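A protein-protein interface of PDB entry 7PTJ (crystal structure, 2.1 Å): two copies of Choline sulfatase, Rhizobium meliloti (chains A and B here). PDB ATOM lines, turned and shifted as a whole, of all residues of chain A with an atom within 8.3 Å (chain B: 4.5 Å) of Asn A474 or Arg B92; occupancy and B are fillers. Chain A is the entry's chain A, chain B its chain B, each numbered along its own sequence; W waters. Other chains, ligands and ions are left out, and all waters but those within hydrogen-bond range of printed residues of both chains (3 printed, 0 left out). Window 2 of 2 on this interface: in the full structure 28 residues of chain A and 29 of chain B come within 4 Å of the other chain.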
ATOM      1  N   ALA A 463     -26.310  -7.062 -22.764  1.00  0.00           N
ATOM      2  CA  ALA A 463     -25.101  -6.329 -22.379  1.00  0.00           C
ATOM      3  C   ALA A 463     -24.411  -5.707 -23.588  1.00  0.00           C
ATOM      4  O   ALA A 463     -23.970  -4.553 -23.536  1.00  0.00           O
ATOM      5  CB  ALA A 463     -24.132  -7.253 -21.641  1.00  0.00           C
ATOM      6  N   ARG A 464     -24.287  -6.465 -24.679  1.00  0.00           N
ATOM      7  CA  ARG A 464     -23.760  -5.905 -25.919  1.00  0.00           C
ATOM      8  C   ARG A 464     -24.468  -4.604 -26.288  1.00  0.00           C
ATOM      9  O   ARG A 464     -23.830  -3.586 -26.602  1.00  0.00           O
ATOM     10  CB  ARG A 464     -23.943  -6.915 -27.044  1.00  0.00           C
ATOM     11  CG  ARG A 464     -22.792  -7.826 -27.323  1.00  0.00           C
ATOM     12  CD  ARG A 464     -23.087  -8.571 -28.626  1.00  0.00           C
ATOM     13  NE  ARG A 464     -22.569  -9.931 -28.605  1.00  0.00           N
ATOM     14  CZ  ARG A 464     -22.617 -10.757 -29.641  1.00  0.00           C
ATOM     15  NH1 ARG A 464     -23.199 -10.404 -30.774  1.00  0.00           N
ATOM     16  NH2 ARG A 464     -22.059 -11.961 -29.539  1.00  0.00           N
ATOM     17  N   ARG A 465     -25.802  -4.636 -26.266  1.00  0.00           N
ATOM     18  CA  ARG A 465     -26.586  -3.528 -26.800  1.00  0.00           C
ATOM     19  C   ARG A 465     -26.540  -2.303 -25.905  1.00  0.00           C
ATOM     20  O   ARG A 465     -26.632  -1.180 -26.402  1.00  0.00           O
ATOM     21  CB  ARG A 465     -28.027  -3.970 -27.021  1.00  0.00           C
ATOM     22  CG  ARG A 465     -28.169  -4.841 -28.246  1.00  0.00           C
ATOM     23  CD  ARG A 465     -29.590  -5.322 -28.377  1.00  0.00           C
ATOM     24  NE  ARG A 465     -29.834  -6.528 -27.597  1.00  0.00           N
ATOM     25  CZ  ARG A 465     -30.990  -6.827 -27.016  1.00  0.00           C
ATOM     26  NH1 ARG A 465     -32.023  -5.997 -27.055  1.00  0.00           N
ATOM     27  NH2 ARG A 465     -31.119  -7.995 -26.395  1.00  0.00           N
ATOM     28  N   TRP A 466     -26.435  -2.477 -24.589  1.00  0.00           N
ATOM     29  CA  TRP A 466     -26.295  -1.310 -23.730  1.00  0.00           C
ATOM     30  C   TRP A 466     -25.043  -0.519 -24.083  1.00  0.00           C
ATOM     31  O   TRP A 466     -25.071   0.715 -24.136  1.00  0.00           O
ATOM     32  CB  TRP A 466     -26.292  -1.737 -22.266  1.00  0.00           C
ATOM     33  CG  TRP A 466     -27.676  -1.968 -21.804  1.00  0.00           C
ATOM     34  CD1 TRP A 466     -28.126  -2.974 -20.993  1.00  0.00           C
ATOM     35  CD2 TRP A 466     -28.824  -1.191 -22.161  1.00  0.00           C
ATOM     36  NE1 TRP A 466     -29.485  -2.860 -20.814  1.00  0.00           N
ATOM     37  CE2 TRP A 466     -29.936  -1.774 -21.522  1.00  0.00           C
ATOM     38  CE3 TRP A 466     -29.019  -0.053 -22.957  1.00  0.00           C
ATOM     39  CZ2 TRP A 466     -31.219  -1.251 -21.641  1.00  0.00           C
ATOM     40  CZ3 TRP A 466     -30.295   0.460 -23.084  1.00  0.00           C
ATOM     41  CH2 TRP A 466     -31.380  -0.137 -22.426  1.00  0.00           C
ATOM     42  N   VAL A 467     -23.937  -1.215 -24.346  1.00  0.00           N
ATOM     43  CA  VAL A 467     -22.736  -0.547 -24.841  1.00  0.00           C
ATOM     44  C   VAL A 467     -23.015   0.104 -26.197  1.00  0.00           C
ATOM     45  O   VAL A 467     -22.808   1.312 -26.397  1.00  0.00           O
ATOM     46  CB  VAL A 467     -21.581  -1.559 -24.936  1.00  0.00           C
ATOM     47  CG1 VAL A 467     -20.336  -0.917 -25.596  1.00  0.00           C
ATOM     48  CG2 VAL A 467     -21.265  -2.122 -23.557  1.00  0.00           C
ATOM     49  N   VAL A 468     -23.509  -0.689 -27.143  1.00  0.00           N
ATOM     50  CA  VAL A 468     -23.581  -0.241 -28.529  1.00  0.00           C
ATOM     51  C   VAL A 468     -24.635   0.849 -28.686  1.00  0.00           C
ATOM     52  O   VAL A 468     -24.388   1.874 -29.326  1.00  0.00           O
ATOM     53  CB  VAL A 468     -23.840  -1.447 -29.459  1.00  0.00           C
ATOM     54  CG1 VAL A 468     -24.348  -1.009 -30.796  1.00  0.00           C
ATOM     55  CG2 VAL A 468     -22.532  -2.273 -29.629  1.00  0.00           C
ATOM     56  N   TYR A 469     -25.826   0.654 -28.103  1.00  0.00           N
ATOM     57  CA  TYR A 469     -26.896   1.628 -28.309  1.00  0.00           C
ATOM     58  C   TYR A 469     -26.528   2.996 -27.738  1.00  0.00           C
ATOM     59  O   TYR A 469     -26.840   4.026 -28.338  1.00  0.00           O
ATOM     60  CB  TYR A 469     -28.213   1.134 -27.707  1.00  0.00           C
ATOM     61  CG  TYR A 469     -29.363   2.060 -28.057  1.00  0.00           C
ATOM     62  CD1 TYR A 469     -29.772   2.218 -29.385  1.00  0.00           C
ATOM     63  CD2 TYR A 469     -30.005   2.817 -27.077  1.00  0.00           C
ATOM     64  CE1 TYR A 469     -30.806   3.083 -29.726  1.00  0.00           C
ATOM     65  CE2 TYR A 469     -31.049   3.691 -27.410  1.00  0.00           C
ATOM     66  CZ  TYR A 469     -31.436   3.815 -28.735  1.00  0.00           C
ATOM     67  OH  TYR A 469     -32.459   4.663 -29.081  1.00  0.00           O
ATOM     68  N   GLU A 470     -25.877   3.036 -26.573  1.00  0.00           N
ATOM     69  CA  GLU A 470     -25.496   4.329 -26.012  1.00  0.00           C
ATOM     70  C   GLU A 470     -24.482   5.032 -26.908  1.00  0.00           C
ATOM     71  O   GLU A 470     -24.507   6.267 -27.038  1.00  0.00           O
ATOM     72  CB  GLU A 470     -24.936   4.165 -24.587  1.00  0.00           C
ATOM     73  CG  GLU A 470     -24.008   5.329 -24.158  1.00  0.00           C
ATOM     74  CD  GLU A 470     -23.519   5.234 -22.692  1.00  0.00           C
ATOM     75  OE1 GLU A 470     -23.587   4.129 -22.089  1.00  0.00           O
ATOM     76  OE2 GLU A 470     -23.041   6.265 -22.158  1.00  0.00           O
ATOM     77  N   ALA A 471     -23.600   4.266 -27.556  1.00  0.00           N
ATOM     78  CA  ALA A 471     -22.669   4.870 -28.501  1.00  0.00           C
ATOM     79  C   ALA A 471     -23.419   5.465 -29.686  1.00  0.00           C
ATOM     80  O   ALA A 471     -23.159   6.608 -30.105  1.00  0.00           O
ATOM     81  CB  ALA A 471     -21.652   3.830 -28.974  1.00  0.00           C
ATOM     82  N   LEU A 472     -24.347   4.687 -30.252  1.00  0.00           N
ATOM     83  CA  LEU A 472     -25.085   5.095 -31.440  1.00  0.00           C
ATOM     84  C   LEU A 472     -25.969   6.310 -31.182  1.00  0.00           C
ATOM     85  O   LEU A 472     -26.306   7.032 -32.128  1.00  0.00           O
ATOM     86  CB  LEU A 472     -25.932   3.934 -31.949  1.00  0.00           C
ATOM     87  CG  LEU A 472     -25.212   2.670 -32.424  1.00  0.00           C
ATOM     88  CD1 LEU A 472     -26.237   1.645 -32.901  1.00  0.00           C
ATOM     89  CD2 LEU A 472     -24.216   3.000 -33.525  1.00  0.00           C
ATOM     90  N   ARG A 473     -26.317   6.579 -29.931  1.00  0.00           N
ATOM     91  CA  ARG A 473     -27.091   7.769 -29.612  1.00  0.00           C
ATOM     92  C   ARG A 473     -26.214   8.966 -29.222  1.00  0.00           C
ATOM     93  O   ARG A 473     -26.743   9.996 -28.792  1.00  0.00           O
ATOM     94  CB  ARG A 473     -28.116   7.443 -28.513  1.00  0.00           C
ATOM     95  CG  ARG A 473     -29.351   6.668 -29.041  1.00  0.00           C
ATOM     96  CD  ARG A 473     -30.227   7.564 -29.948  1.00  0.00           C
ATOM     97  NE  ARG A 473     -31.356   6.855 -30.546  1.00  0.00           N
ATOM     98  CZ  ARG A 473     -32.095   7.325 -31.548  1.00  0.00           C
ATOM     99  NH1 ARG A 473     -31.885   8.527 -32.065  1.00  0.00           N
ATOM    100  NH2 ARG A 473     -33.061   6.566 -32.056  1.00  0.00           N
ATOM    101  N   ASN A 474     -24.895   8.855 -29.379  1.00  0.00           N
ATOM    102  CA  ASN A 474     -23.994   9.995 -29.289  1.00  0.00           C
ATOM    103  C   ASN A 474     -23.729  10.539 -30.688  1.00  0.00           C
ATOM    104  O   ASN A 474     -23.557   9.771 -31.638  1.00  0.00           O
ATOM    105  CB  ASN A 474     -22.678   9.611 -28.623  1.00  0.00           C
ATOM    106  CG  ASN A 474     -22.807   9.489 -27.108  1.00  0.00           C
ATOM    107  OD1 ASN A 474     -23.821   9.863 -26.539  1.00  0.00           O
ATOM    108  ND2 ASN A 474     -21.794   8.952 -26.464  1.00  0.00           N
ATOM    109  N   GLY A 475     -23.703  11.872 -30.808  1.00  0.00           N
ATOM    110  CA  GLY A 475     -23.419  12.485 -32.091  1.00  0.00           C
ATOM    111  C   GLY A 475     -24.581  12.323 -33.063  1.00  0.00           C
ATOM    112  O   GLY A 475     -25.742  12.135 -32.682  1.00  0.00           O
ATOM    113  N   ALA A 476     -24.248  12.413 -34.347  1.00  0.00           N
ATOM    114  CA  ALA A 476     -25.257  12.296 -35.392  1.00  0.00           C
ATOM    115  C   ALA A 476     -25.800  10.869 -35.450  1.00  0.00           C
ATOM    116  O   ALA A 476     -25.032   9.899 -35.523  1.00  0.00           O
ATOM    117  CB  ALA A 476     -24.666  12.690 -36.748  1.00  0.00           C
ATOM    118  N   TYR A 477     -27.125  10.745 -35.429  1.00  0.00           N
ATOM    119  CA  TYR A 477     -27.765   9.444 -35.502  1.00  0.00           C
ATOM    120  C   TYR A 477     -27.829   8.959 -36.949  1.00  0.00           C
ATOM    121  O   TYR A 477     -28.132   9.730 -37.857  1.00  0.00           O
ATOM    122  CB  TYR A 477     -29.178   9.512 -34.909  1.00  0.00           C
ATOM    123  CG  TYR A 477     -29.785   8.140 -34.746  1.00  0.00           C
ATOM    124  CD1 TYR A 477     -29.144   7.164 -33.981  1.00  0.00           C
ATOM    125  CD2 TYR A 477     -30.972   7.800 -35.387  1.00  0.00           C
ATOM    126  CE1 TYR A 477     -29.678   5.900 -33.842  1.00  0.00           C
ATOM    127  CE2 TYR A 477     -31.528   6.530 -35.242  1.00  0.00           C
ATOM    128  CZ  TYR A 477     -30.874   5.588 -34.470  1.00  0.00           C
ATOM    129  OH  TYR A 477     -31.401   4.329 -34.348  1.00  0.00           O
ATOM    130  N   TYR A 478     -27.534   7.680 -37.167  1.00  0.00           N
ATOM    131  CA  TYR A 478     -27.773   7.063 -38.477  1.00  0.00           C
ATOM    132  C   TYR A 478     -28.996   6.152 -38.416  1.00  0.00           C
ATOM    133  O   TYR A 478     -28.911   5.047 -37.846  1.00  0.00           O
ATOM    134  CB  TYR A 478     -26.552   6.267 -38.939  1.00  0.00           C
ATOM    135  CG  TYR A 478     -26.614   5.832 -40.400  1.00  0.00           C
ATOM    136  CD1 TYR A 478     -26.213   6.698 -41.420  1.00  0.00           C
ATOM    137  CD2 TYR A 478     -27.047   4.554 -40.758  1.00  0.00           C
ATOM    138  CE1 TYR A 478     -26.249   6.305 -42.754  1.00  0.00           C
ATOM    139  CE2 TYR A 478     -27.087   4.154 -42.092  1.00  0.00           C
ATOM    140  CZ  TYR A 478     -26.688   5.038 -43.081  1.00  0.00           C
ATOM    141  OH  TYR A 478     -26.711   4.652 -44.403  1.00  0.00           O
ATOM    142  N   HIS B  88     -17.501   2.253 -31.335  1.00  0.00           N
ATOM    143  CA  HIS B  88     -18.483   2.378 -30.252  1.00  0.00           C
ATOM    144  C   HIS B  88     -17.812   2.830 -28.961  1.00  0.00           C
ATOM    145  O   HIS B  88     -18.329   3.698 -28.245  1.00  0.00           O
ATOM    146  CB  HIS B  88     -19.206   1.055 -29.984  1.00  0.00           C
ATOM    147  CG  HIS B  88     -20.014   0.530 -31.126  1.00  0.00           C
ATOM    148  ND1 HIS B  88     -19.575  -0.509 -31.919  1.00  0.00           N
ATOM    149  CD2 HIS B  88     -21.259   0.842 -31.570  1.00  0.00           C
ATOM    150  CE1 HIS B  88     -20.491  -0.776 -32.839  1.00  0.00           C
ATOM    151  NE2 HIS B  88     -21.526   0.023 -32.645  1.00  0.00           N
ATOM    152  N   HIS B  89     -16.667   2.221 -28.625  1.00  0.00           N
ATOM    153  CA  HIS B  89     -16.034   2.522 -27.345  1.00  0.00           C
ATOM    154  C   HIS B  89     -15.615   3.991 -27.287  1.00  0.00           C
ATOM    155  O   HIS B  89     -15.873   4.686 -26.297  1.00  0.00           O
ATOM    156  CB  HIS B  89     -14.820   1.616 -27.117  1.00  0.00           C
ATOM    157  CG  HIS B  89     -15.129   0.150 -26.985  1.00  0.00           C
ATOM    158  ND1 HIS B  89     -16.023  -0.355 -26.061  1.00  0.00           N
ATOM    159  CD2 HIS B  89     -14.608  -0.924 -27.627  1.00  0.00           C
ATOM    160  CE1 HIS B  89     -16.049  -1.674 -26.151  1.00  0.00           C
ATOM    161  NE2 HIS B  89     -15.191  -2.047 -27.086  1.00  0.00           N
ATOM    162  N   LEU B  90     -14.968   4.482 -28.346  1.00  0.00           N
ATOM    163  CA  LEU B  90     -14.567   5.891 -28.392  1.00  0.00           C
ATOM    164  C   LEU B  90     -15.773   6.819 -28.427  1.00  0.00           C
ATOM    165  O   LEU B  90     -15.811   7.839 -27.724  1.00  0.00           O
ATOM    166  CB  LEU B  90     -13.690   6.145 -29.616  1.00  0.00           C
ATOM    167  CG  LEU B  90     -12.347   5.436 -29.549  1.00  0.00           C
ATOM    168  CD1 LEU B  90     -11.525   5.657 -30.817  1.00  0.00           C
ATOM    169  CD2 LEU B  90     -11.641   5.947 -28.324  1.00  0.00           C
ATOM    170  N   ARG B  91     -16.748   6.502 -29.284  1.00  0.00           N
ATOM    171  CA  ARG B  91     -17.938   7.336 -29.424  1.00  0.00           C
ATOM    172  C   ARG B  91     -18.669   7.455 -28.096  1.00  0.00           C
ATOM    173  O   ARG B  91     -19.108   8.549 -27.705  1.00  0.00           O
ATOM    174  CB  ARG B  91     -18.836   6.733 -30.506  1.00  0.00           C
ATOM    175  CG  ARG B  91     -20.089   7.470 -30.826  1.00  0.00           C
ATOM    176  CD  ARG B  91     -20.766   6.809 -32.027  1.00  0.00           C
ATOM    177  NE  ARG B  91     -21.868   7.600 -32.562  1.00  0.00           N
ATOM    178  CZ  ARG B  91     -22.580   7.261 -33.633  1.00  0.00           C
ATOM    179  NH1 ARG B  91     -22.306   6.162 -34.325  1.00  0.00           N
ATOM    180  NH2 ARG B  91     -23.594   8.036 -34.013  1.00  0.00           N
ATOM    181  N   ARG B  92     -18.775   6.333 -27.380  1.00  0.00           N
ATOM    182  CA  ARG B  92     -19.366   6.312 -26.049  1.00  0.00           C
ATOM    183  C   ARG B  92     -18.598   7.195 -25.079  1.00  0.00           C
ATOM    184  O   ARG B  92     -19.188   7.742 -24.138  1.00  0.00           O
ATOM    185  CB  ARG B  92     -19.396   4.869 -25.522  1.00  0.00           C
ATOM    186  CG  ARG B  92     -20.423   4.602 -24.459  1.00  0.00           C
ATOM    187  CD  ARG B  92     -20.445   3.116 -24.072  1.00  0.00           C
ATOM    188  NE  ARG B  92     -20.868   2.949 -22.688  1.00  0.00           N
ATOM    189  CZ  ARG B  92     -20.279   2.152 -21.810  1.00  0.00           C
ATOM    190  NH1 ARG B  92     -19.245   1.394 -22.150  1.00  0.00           N
ATOM    191  NH2 ARG B  92     -20.728   2.125 -20.558  1.00  0.00           N
ATOM    192  N   ALA B  93     -17.281   7.311 -25.257  1.00  0.00           N
ATOM    193  CA  ALA B  93     -16.467   8.148 -24.383  1.00  0.00           C
ATOM    194  C   ALA B  93     -16.471   9.621 -24.789  1.00  0.00           C
ATOM    195  O   ALA B  93     -15.816  10.427 -24.121  1.00  0.00           O
ATOM    196  CB  ALA B  93     -15.023   7.630 -24.343  1.00  0.00           C
ATOM    197  N   GLY B  94     -17.174   9.992 -25.856  1.00  0.00           N
ATOM    198  CA  GLY B  94     -17.278  11.381 -26.270  1.00  0.00           C
ATOM    199  C   GLY B  94     -16.533  11.767 -27.534  1.00  0.00           C
ATOM    200  O   GLY B  94     -16.420  12.969 -27.817  1.00  0.00           O
ATOM    201  N   GLU B 115     -19.450   7.143 -36.598  1.00  0.00           N
ATOM    202  CA  GLU B 115     -20.488   8.155 -36.693  1.00  0.00           C
ATOM    203  C   GLU B 115     -20.664   8.620 -38.131  1.00  0.00           C
ATOM    204  O   GLU B 115     -21.782   8.938 -38.548  1.00  0.00           O
ATOM    205  CB  GLU B 115     -20.165   9.330 -35.765  1.00  0.00           C
ATOM    206  CG  GLU B 115     -21.080  10.506 -35.916  1.00  0.00           C
ATOM    207  CD  GLU B 115     -20.953  11.485 -34.767  1.00  0.00           C
ATOM    208  OE1 GLU B 115     -20.280  11.130 -33.774  1.00  0.00           O
ATOM    209  OE2 GLU B 115     -21.525  12.603 -34.858  1.00  0.00           O
ATOM    210  N   GLU B 356     -14.226  -1.327 -18.563  1.00  0.00           N
ATOM    211  CA  GLU B 356     -15.278  -1.064 -19.539  1.00  0.00           C
ATOM    212  C   GLU B 356     -15.069  -1.836 -20.831  1.00  0.00           C
ATOM    213  O   GLU B 356     -16.045  -2.145 -21.524  1.00  0.00           O
ATOM    214  CB  GLU B 356     -15.378   0.431 -19.828  1.00  0.00           C
ATOM    215  CG  GLU B 356     -16.411   1.104 -18.946  1.00  0.00           C
ATOM    216  CD  GLU B 356     -16.430   2.598 -19.114  1.00  0.00           C
ATOM    217  OE1 GLU B 356     -15.418   3.248 -18.756  1.00  0.00           O
ATOM    218  OE2 GLU B 356     -17.439   3.122 -19.635  1.00  0.00           O
HETATM  219  O   HOH W   1     -26.135   6.366 -34.974  1.00  0.00           O
HETATM  220  O   HOH W   2     -22.068   8.051 -23.547  1.00  0.00           O
HETATM  221  O   HOH W   3     -24.221   8.383 -37.371  1.00  0.00           O
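The backbone NH (N) of Ala A476 is in hydrogen-bond range of the side-chain carboxylate (OE2) of Glu B115 (2.8 Å).
The backbone carbonyl oxygen (O) of Ala A471 is in hydrogen-bond range of the guanidinium group (NE) of Arg B91 (2.9 Å).
The guanidinium group of Arg B92 lies within salt-bridge range of the side-chain carboxylate of Glu A470, 3.0 Å away.
The backbone carbonyl oxygen (O) of Leu A472 sits at hydrogen-bond distance from the guanidinium group (NH2) of Arg B91 (3.5 Å).
O of Ala A476 lies within hydrogen-bond range of NH2 of Arg B91, at 2.8 Å.
The backbone carbonyl oxygen (O) of Asn A474 sits at hydrogen-bond distance from the guanidinium group (NE) of Arg B91.
The side-chain carboxylate (OE2) of Glu B356 is in salt-bridge range of the guanidinium group (NH1) of Arg B92.
Among the printed residues, pairs that only touch across the chains: Gly A475 with Glu B115 (3.4 Å), Ala A471 with His B88 (3.4 Å), Val A468 with His B88 (3.5 Å), Asn A474 with Arg B92 (3.6 Å) and Val A467 with Arg B92 (3.8 Å).
Of the printed residues of chain B, Val A468 touches His B88.
Of the printed residues of chain B, Glu A470 touches Arg B92 (3.0 Å).
Of the printed residues of chain B, Ala A471 touches His B88 (3.4 Å) and Arg B91 (2.9 Å).
Of chain B, only Arg B91 (2.9 Å) and Arg B92 (3.6 Å) come within 4 Å of Asn A474.
Printed residues of chain A within 4 Å of Arg B91: Ala A471, Leu A472, Asn A474 and Ala A476.
Of chain A, only Val A467, Glu A470 and Asn A474 come within 4 Å of Arg B92.
Of the printed residues of chain A, Glu B115 touches Gly A475 (3.4 Å) and Ala A476 (2.8 Å).
Glu B356 touches none of the printed residues of chain A.
The nearest residue of chain A that does not touch Arg B92 is Ala A471 (4.1 Å).
Printed residues of chain A that touch a printed residue of chain B: Val A467, Val A468, Glu A470, Ala A471, Leu A472, Asn A474, Gly A475 and Ala A476.
Hydrophobic or aromatic side chains of chain A within 4 Å of the printed part of chain B: Val A468, Ala A471, Leu A472 and Ala A476.
Of the 9 printed residues of chain B, 4 touch a printed residue of chain A.
No position is printed for both chains.
Of the 11 pairs that touch across the chains among the printed residues, none has its exchanged pair printed and touching as well.
Water W2 lies within hydrogen-bond range of OE2 of Glu A470 (2.5 Å), O of Arg B92 (3.0 Å) and ND2 of Asn A474 (3.1 Å).
Water W3 lies within hydrogen-bond range of the backbone carbonyl oxygen of Ala A476 (2.5 Å), the backbone carbonyl oxygen of Glu B115 (2.8 Å), the backbone NH of Tyr A478 (3.4 Å) and the guanidinium group of Arg B91 (3.4 Å).
Water W1 lies within hydrogen-bond range of the backbone NH of Tyr A478, the backbone carbonyl oxygen of Leu A472 and the guanidinium group of Arg B91.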
